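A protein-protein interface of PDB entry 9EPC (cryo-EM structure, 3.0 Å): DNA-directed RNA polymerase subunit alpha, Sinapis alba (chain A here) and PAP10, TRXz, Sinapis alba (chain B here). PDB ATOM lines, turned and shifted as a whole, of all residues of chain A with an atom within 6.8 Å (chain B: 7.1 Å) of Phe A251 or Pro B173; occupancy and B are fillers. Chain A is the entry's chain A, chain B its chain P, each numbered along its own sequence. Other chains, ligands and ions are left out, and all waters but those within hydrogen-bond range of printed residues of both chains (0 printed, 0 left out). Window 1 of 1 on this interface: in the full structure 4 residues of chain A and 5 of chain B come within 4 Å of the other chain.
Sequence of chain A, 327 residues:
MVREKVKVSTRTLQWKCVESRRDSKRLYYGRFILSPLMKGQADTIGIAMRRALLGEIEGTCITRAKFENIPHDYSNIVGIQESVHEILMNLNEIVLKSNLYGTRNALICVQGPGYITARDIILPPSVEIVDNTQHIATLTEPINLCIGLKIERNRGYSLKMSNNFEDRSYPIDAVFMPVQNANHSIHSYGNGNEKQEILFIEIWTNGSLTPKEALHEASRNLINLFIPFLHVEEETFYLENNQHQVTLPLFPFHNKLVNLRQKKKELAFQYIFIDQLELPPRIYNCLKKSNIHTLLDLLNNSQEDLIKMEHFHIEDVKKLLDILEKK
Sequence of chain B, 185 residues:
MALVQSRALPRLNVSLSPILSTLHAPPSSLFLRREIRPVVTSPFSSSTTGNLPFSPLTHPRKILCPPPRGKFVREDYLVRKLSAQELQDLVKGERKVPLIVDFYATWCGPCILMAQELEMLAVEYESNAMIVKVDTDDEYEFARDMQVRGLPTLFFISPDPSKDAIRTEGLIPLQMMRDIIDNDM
Printed residues of chain A that touch a printed residue of chain B: Leu A248, Phe A251 and His A254.
Along chain A the printed residues that touch a printed residue of chain B span positions 248 to 254.
Among the printed residues, no Asp or Glu carboxylate lies within 4 Å of a Lys or Arg side-chain nitrogen of the other chain.
The backbone carbonyl oxygen (O) of Ile B172 lies close to the side-chain carboxylate (OE1) of Glu B117.
Of chain B, only Glu B117 (3.0 Å), Leu B171 (3.3 Å), Ile B172 (3.7 Å) and Pro B173 (3.6 Å) come within 4 Å of Phe A251.
Of the printed residues of chain B, His A254 touches Pro B173 (3.6 Å).
Printed residues of chain A within 4 Å of Ile B172: Phe A251 (3.7 Å).
Of the printed residues of chain B, Leu A248 touches Leu B171.
The nearest residue of chain B that does not touch Phe A251 is Leu B174 (5.1 Å).
The nearest residue of chain A that does not touch Pro B173 is Leu A250 (5.8 Å).
The nearest printed residue of chain A that does not touch Ile B172 is Leu A248 (6.6 Å).
Among the printed residues, pairs that only touch across the chains: Phe A251 with Glu B117, Phe A251 with Leu B171, His A254 with Pro B173, Leu A248 with Leu B171, Phe A251 with Pro B173 and Phe A251 with Ile B172.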
ATOM      1  N   TYR A 238      26.844  29.599  23.453  1.00  0.00           N
ATOM      2  CA  TYR A 238      26.042  30.071  24.569  1.00  0.00           C
ATOM      3  C   TYR A 238      24.969  29.048  24.923  1.00  0.00           C
ATOM      4  O   TYR A 238      24.407  28.377  24.055  1.00  0.00           O
ATOM      5  CB  TYR A 238      25.396  31.415  24.238  1.00  0.00           C
ATOM      6  CG  TYR A 238      24.445  31.902  25.304  1.00  0.00           C
ATOM      7  CD1 TYR A 238      24.915  32.561  26.430  1.00  0.00           C
ATOM      8  CD2 TYR A 238      23.078  31.693  25.191  1.00  0.00           C
ATOM      9  CE1 TYR A 238      24.050  33.003  27.409  1.00  0.00           C
ATOM     10  CE2 TYR A 238      22.207  32.130  26.164  1.00  0.00           C
ATOM     11  CZ  TYR A 238      22.697  32.785  27.272  1.00  0.00           C
ATOM     12  OH  TYR A 238      21.831  33.223  28.244  1.00  0.00           O
ATOM     13  N   VAL A 246      22.431  20.662  23.710  1.00  0.00           N
ATOM     14  CA  VAL A 246      21.537  21.267  22.732  1.00  0.00           C
ATOM     15  C   VAL A 246      21.786  20.619  21.380  1.00  0.00           C
ATOM     16  O   VAL A 246      22.930  20.551  20.916  1.00  0.00           O
ATOM     17  CB  VAL A 246      21.729  22.791  22.662  1.00  0.00           C
ATOM     18  CG1 VAL A 246      21.029  23.460  23.830  1.00  0.00           C
ATOM     19  CG2 VAL A 246      23.208  23.139  22.666  1.00  0.00           C
ATOM     20  N   THR A 247      20.713  20.128  20.755  1.00  0.00           N
ATOM     21  CA  THR A 247      20.842  19.537  19.429  1.00  0.00           C
ATOM     22  C   THR A 247      21.280  20.576  18.407  1.00  0.00           C
ATOM     23  O   THR A 247      22.124  20.299  17.549  1.00  0.00           O
ATOM     24  CB  THR A 247      19.520  18.900  19.006  1.00  0.00           C
ATOM     25  OG1 THR A 247      18.547  19.928  18.789  1.00  0.00           O
ATOM     26  CG2 THR A 247      19.020  17.970  20.088  1.00  0.00           C
ATOM     27  N   LEU A 248      20.716  21.778  18.483  1.00  0.00           N
ATOM     28  CA  LEU A 248      21.081  22.869  17.588  1.00  0.00           C
ATOM     29  C   LEU A 248      21.768  23.960  18.392  1.00  0.00           C
ATOM     30  O   LEU A 248      21.098  24.719  19.106  1.00  0.00           O
ATOM     31  CB  LEU A 248      19.842  23.419  16.880  1.00  0.00           C
ATOM     32  CG  LEU A 248      19.066  22.360  16.101  1.00  0.00           C
ATOM     33  CD1 LEU A 248      17.835  22.963  15.477  1.00  0.00           C
ATOM     34  CD2 LEU A 248      19.947  21.738  15.038  1.00  0.00           C
ATOM     35  N   PRO A 249      23.094  24.081  18.317  1.00  0.00           N
ATOM     36  CA  PRO A 249      23.794  25.049  19.176  1.00  0.00           C
ATOM     37  C   PRO A 249      23.442  26.495  18.889  1.00  0.00           C
ATOM     38  O   PRO A 249      23.685  27.354  19.743  1.00  0.00           O
ATOM     39  CB  PRO A 249      25.273  24.764  18.885  1.00  0.00           C
ATOM     40  CG  PRO A 249      25.275  24.158  17.526  1.00  0.00           C
ATOM     41  CD  PRO A 249      24.018  23.353  17.432  1.00  0.00           C
ATOM     42  N   LEU A 250      22.886  26.796  17.718  1.00  0.00           N
ATOM     43  CA  LEU A 250      22.563  28.178  17.385  1.00  0.00           C
ATOM     44  C   LEU A 250      21.342  28.686  18.139  1.00  0.00           C
ATOM     45  O   LEU A 250      21.295  29.865  18.508  1.00  0.00           O
ATOM     46  CB  LEU A 250      22.342  28.310  15.880  1.00  0.00           C
ATOM     47  CG  LEU A 250      21.869  29.669  15.371  1.00  0.00           C
ATOM     48  CD1 LEU A 250      22.746  30.125  14.232  1.00  0.00           C
ATOM     49  CD2 LEU A 250      20.421  29.593  14.925  1.00  0.00           C
ATOM     50  N   PHE A 251      20.355  27.826  18.375  1.00  0.00           N
ATOM     51  CA  PHE A 251      19.092  28.278  18.957  1.00  0.00           C
ATOM     52  C   PHE A 251      19.232  28.893  20.344  1.00  0.00           C
ATOM     53  O   PHE A 251      18.611  29.943  20.587  1.00  0.00           O
ATOM     54  CB  PHE A 251      18.088  27.124  18.959  1.00  0.00           C
ATOM     55  CG  PHE A 251      17.460  26.877  17.624  1.00  0.00           C
ATOM     56  CD1 PHE A 251      17.837  27.623  16.521  1.00  0.00           C
ATOM     57  CD2 PHE A 251      16.485  25.916  17.470  1.00  0.00           C
ATOM     58  CE1 PHE A 251      17.261  27.403  15.293  1.00  0.00           C
ATOM     59  CE2 PHE A 251      15.905  25.696  16.244  1.00  0.00           C
ATOM     60  CZ  PHE A 251      16.293  26.439  15.155  1.00  0.00           C
ATOM     61  N   PRO A 252      19.981  28.318  21.293  1.00  0.00           N
ATOM     62  CA  PRO A 252      20.055  28.950  22.621  1.00  0.00           C
ATOM     63  C   PRO A 252      20.576  30.375  22.587  1.00  0.00           C
ATOM     64  O   PRO A 252      20.172  31.188  23.424  1.00  0.00           O
ATOM     65  CB  PRO A 252      20.995  28.021  23.403  1.00  0.00           C
ATOM     66  CG  PRO A 252      21.721  27.247  22.371  1.00  0.00           C
ATOM     67  CD  PRO A 252      20.740  27.058  21.267  1.00  0.00           C
ATOM     68  N   PHE A 253      21.463  30.706  21.646  1.00  0.00           N
ATOM     69  CA  PHE A 253      21.883  32.095  21.512  1.00  0.00           C
ATOM     70  C   PHE A 253      20.789  32.952  20.894  1.00  0.00           C
ATOM     71  O   PHE A 253      20.658  34.129  21.242  1.00  0.00           O
ATOM     72  CB  PHE A 253      23.157  32.192  20.680  1.00  0.00           C
ATOM     73  CG  PHE A 253      23.721  33.578  20.606  1.00  0.00           C
ATOM     74  CD1 PHE A 253      24.538  34.057  21.612  1.00  0.00           C
ATOM     75  CD2 PHE A 253      23.432  34.404  19.536  1.00  0.00           C
ATOM     76  CE1 PHE A 253      25.058  35.329  21.550  1.00  0.00           C
ATOM     77  CE2 PHE A 253      23.950  35.677  19.470  1.00  0.00           C
ATOM     78  CZ  PHE A 253      24.764  36.140  20.479  1.00  0.00           C
ATOM     79  N   HIS A 254      20.010  32.392  19.968  1.00  0.00           N
ATOM     80  CA  HIS A 254      18.890  33.141  19.408  1.00  0.00           C
ATOM     81  C   HIS A 254      17.859  33.460  20.480  1.00  0.00           C
ATOM     82  O   HIS A 254      17.299  34.561  20.506  1.00  0.00           O
ATOM     83  CB  HIS A 254      18.245  32.361  18.265  1.00  0.00           C
ATOM     84  CG  HIS A 254      17.059  33.048  17.665  1.00  0.00           C
ATOM     85  ND1 HIS A 254      15.774  32.843  18.118  1.00  0.00           N
ATOM     86  CD2 HIS A 254      16.965  33.942  16.654  1.00  0.00           C
ATOM     87  CE1 HIS A 254      14.938  33.578  17.407  1.00  0.00           C
ATOM     88  NE2 HIS A 254      15.635  34.255  16.514  1.00  0.00           N
ATOM     89  N   ASN A 255      17.593  32.505  21.373  1.00  0.00           N
ATOM     90  CA  ASN A 255      16.693  32.763  22.489  1.00  0.00           C
ATOM     91  C   ASN A 255      17.224  33.855  23.404  1.00  0.00           C
ATOM     92  O   ASN A 255      16.439  34.503  24.101  1.00  0.00           O
ATOM     93  CB  ASN A 255      16.460  31.478  23.283  1.00  0.00           C
ATOM     94  CG  ASN A 255      15.438  31.654  24.384  1.00  0.00           C
ATOM     95  OD1 ASN A 255      15.780  31.990  25.516  1.00  0.00           O
ATOM     96  ND2 ASN A 255      14.171  31.429  24.055  1.00  0.00           N
ATOM     97  N   LYS A 256      18.539  34.069  23.420  1.00  0.00           N
ATOM     98  CA  LYS A 256      19.095  35.176  24.189  1.00  0.00           C
ATOM     99  C   LYS A 256      18.793  36.512  23.525  1.00  0.00           C
ATOM    100  O   LYS A 256      18.435  37.481  24.203  1.00  0.00           O
ATOM    101  CB  LYS A 256      20.600  34.992  24.360  1.00  0.00           C
ATOM    102  CG  LYS A 256      21.281  36.126  25.095  1.00  0.00           C
ATOM    103  CD  LYS A 256      22.786  35.950  25.102  1.00  0.00           C
ATOM    104  CE  LYS A 256      23.459  37.056  25.888  1.00  0.00           C
ATOM    105  NZ  LYS A 256      23.038  37.050  27.315  1.00  0.00           N
ATOM    106  N   MET B 114      12.374  20.061  11.874  1.00  0.00           N
ATOM    107  CA  MET B 114      11.413  21.104  11.536  1.00  0.00           C
ATOM    108  C   MET B 114       9.994  20.686  11.887  1.00  0.00           C
ATOM    109  O   MET B 114       9.176  21.530  12.268  1.00  0.00           O
ATOM    110  CB  MET B 114      11.522  21.441  10.049  1.00  0.00           C
ATOM    111  CG  MET B 114      10.490  22.425   9.525  1.00  0.00           C
ATOM    112  SD  MET B 114      11.098  24.119   9.418  1.00  0.00           S
ATOM    113  CE  MET B 114      10.881  24.670  11.105  1.00  0.00           C
ATOM    114  N   GLU B 117       9.126  21.266  15.749  1.00  0.00           N
ATOM    115  CA  GLU B 117       8.746  22.645  16.040  1.00  0.00           C
ATOM    116  C   GLU B 117       7.318  22.921  15.593  1.00  0.00           C
ATOM    117  O   GLU B 117       6.545  23.569  16.306  1.00  0.00           O
ATOM    118  CB  GLU B 117       9.715  23.608  15.364  1.00  0.00           C
ATOM    119  CG  GLU B 117      11.138  23.494  15.850  1.00  0.00           C
ATOM    120  CD  GLU B 117      12.043  24.482  15.160  1.00  0.00           C
ATOM    121  OE1 GLU B 117      11.576  25.134  14.207  1.00  0.00           O
ATOM    122  OE2 GLU B 117      13.212  24.613  15.568  1.00  0.00           O
ATOM    123  N   LEU B 154       9.464  26.546   4.549  1.00  0.00           N
ATOM    124  CA  LEU B 154       8.154  26.888   5.078  1.00  0.00           C
ATOM    125  C   LEU B 154       7.569  28.051   4.294  1.00  0.00           C
ATOM    126  O   LEU B 154       8.263  29.030   4.005  1.00  0.00           O
ATOM    127  CB  LEU B 154       8.226  27.256   6.558  1.00  0.00           C
ATOM    128  CG  LEU B 154       8.650  26.151   7.520  1.00  0.00           C
ATOM    129  CD1 LEU B 154       8.542  26.645   8.945  1.00  0.00           C
ATOM    130  CD2 LEU B 154       7.797  24.919   7.313  1.00  0.00           C
ATOM    131  N   GLY B 170      15.658  26.911   5.600  1.00  0.00           N
ATOM    132  CA  GLY B 170      16.492  26.533   6.719  1.00  0.00           C
ATOM    133  C   GLY B 170      15.672  26.229   7.958  1.00  0.00           C
ATOM    134  O   GLY B 170      14.482  26.536   8.058  1.00  0.00           O
ATOM    135  N   LEU B 171      16.337  25.608   8.924  1.00  0.00           N
ATOM    136  CA  LEU B 171      15.697  25.213  10.176  1.00  0.00           C
ATOM    137  C   LEU B 171      15.508  26.464  11.023  1.00  0.00           C
ATOM    138  O   LEU B 171      16.340  26.809  11.861  1.00  0.00           O
ATOM    139  CB  LEU B 171      16.533  24.161  10.888  1.00  0.00           C
ATOM    140  CG  LEU B 171      15.871  23.387  12.022  1.00  0.00           C
ATOM    141  CD1 LEU B 171      14.417  23.132  11.695  1.00  0.00           C
ATOM    142  CD2 LEU B 171      16.597  22.079  12.224  1.00  0.00           C
ATOM    143  N   ILE B 172      14.398  27.156  10.789  1.00  0.00           N
ATOM    144  CA  ILE B 172      14.100  28.424  11.451  1.00  0.00           C
ATOM    145  C   ILE B 172      13.714  28.153  12.902  1.00  0.00           C
ATOM    146  O   ILE B 172      13.178  27.078  13.208  1.00  0.00           O
ATOM    147  CB  ILE B 172      12.997  29.187  10.694  1.00  0.00           C
ATOM    148  CG1 ILE B 172      13.380  30.655  10.514  1.00  0.00           C
ATOM    149  CG2 ILE B 172      11.668  29.083  11.406  1.00  0.00           C
ATOM    150  CD1 ILE B 172      14.672  30.856   9.766  1.00  0.00           C
ATOM    151  N   PRO B 173      13.993  29.068  13.831  1.00  0.00           N
ATOM    152  CA  PRO B 173      13.597  28.849  15.224  1.00  0.00           C
ATOM    153  C   PRO B 173      12.105  29.041  15.430  1.00  0.00           C
ATOM    154  O   PRO B 173      11.408  29.670  14.631  1.00  0.00           O
ATOM    155  CB  PRO B 173      14.395  29.908  15.988  1.00  0.00           C
ATOM    156  CG  PRO B 173      14.602  30.981  14.995  1.00  0.00           C
ATOM    157  CD  PRO B 173      14.825  30.272  13.692  1.00  0.00           C
ATOM    158  N   LEU B 174      11.622  28.496  16.547  1.00  0.00           N
ATOM    159  CA  LEU B 174      10.198  28.561  16.850  1.00  0.00           C
ATOM    160  C   LEU B 174       9.743  29.993  17.091  1.00  0.00           C
ATOM    161  O   LEU B 174       8.638  30.377  16.691  1.00  0.00           O
ATOM    162  CB  LEU B 174       9.883  27.697  18.067  1.00  0.00           C
ATOM    163  CG  LEU B 174       8.398  27.521  18.367  1.00  0.00           C
ATOM    164  CD1 LEU B 174       7.799  26.455  17.474  1.00  0.00           C
ATOM    165  CD2 LEU B 174       8.192  27.179  19.823  1.00  0.00           C
ATOM    166  N   GLN B 175      10.580  30.796  17.751  1.00  0.00           N
ATOM    167  CA  GLN B 175      10.176  32.151  18.121  1.00  0.00           C
ATOM    168  C   GLN B 175       9.895  33.006  16.893  1.00  0.00           C
ATOM    169  O   GLN B 175       8.946  33.797  16.886  1.00  0.00           O
ATOM    170  CB  GLN B 175      11.249  32.803  18.990  1.00  0.00           C
ATOM    171  CG  GLN B 175      10.985  34.270  19.297  1.00  0.00           C
ATOM    172  CD  GLN B 175       9.629  34.501  19.941  1.00  0.00           C
ATOM    173  OE1 GLN B 175       9.150  33.680  20.722  1.00  0.00           O
ATOM    174  NE2 GLN B 175       9.002  35.623  19.609  1.00  0.00           N
ATOM    175  N   MET B 176      10.715  32.873  15.851  1.00  0.00           N
ATOM    176  CA  MET B 176      10.507  33.686  14.658  1.00  0.00           C
ATOM    177  C   MET B 176       9.186  33.350  13.985  1.00  0.00           C
ATOM    178  O   MET B 176       8.498  34.240  13.475  1.00  0.00           O
ATOM    179  CB  MET B 176      11.663  33.503  13.682  1.00  0.00           C
ATOM    180  CG  MET B 176      11.643  34.500  12.540  1.00  0.00           C
ATOM    181  SD  MET B 176      12.912  34.117  11.332  1.00  0.00           S
ATOM    182  CE  MET B 176      14.210  33.624  12.452  1.00  0.00           C
ATOM    183  N   MET B 177       8.813  32.069  13.971  1.00  0.00           N
ATOM    184  CA  MET B 177       7.523  31.690  13.407  1.00  0.00           C
ATOM    185  C   MET B 177       6.370  32.326  14.167  1.00  0.00           C
ATOM    186  O   MET B 177       5.305  32.565  13.588  1.00  0.00           O
ATOM    187  CB  MET B 177       7.372  30.171  13.401  1.00  0.00           C
ATOM    188  CG  MET B 177       8.308  29.468  12.446  1.00  0.00           C
ATOM    189  SD  MET B 177       7.936  27.717  12.270  1.00  0.00           S
ATOM    190  CE  MET B 177       8.325  27.125  13.910  1.00  0.00           C
ATOM    191  N   ARG B 178       6.555  32.600  15.460  1.00  0.00           N
ATOM    192  CA  ARG B 178       5.509  33.268  16.225  1.00  0.00           C
ATOM    193  C   ARG B 178       5.241  34.663  15.680  1.00  0.00           C
ATOM    194  O   ARG B 178       4.096  35.012  15.371  1.00  0.00           O
ATOM    195  CB  ARG B 178       5.898  33.343  17.699  1.00  0.00           C
ATOM    196  CG  ARG B 178       5.832  32.028  18.441  1.00  0.00           C
ATOM    197  CD  ARG B 178       6.022  32.266  19.925  1.00  0.00           C
ATOM    198  NE  ARG B 178       5.863  31.050  20.711  1.00  0.00           N
ATOM    199  CZ  ARG B 178       6.868  30.293  21.126  1.00  0.00           C
ATOM    200  NH1 ARG B 178       8.123  30.590  20.835  1.00  0.00           N
ATOM    201  NH2 ARG B 178       6.608  29.214  21.859  1.00  0.00           N
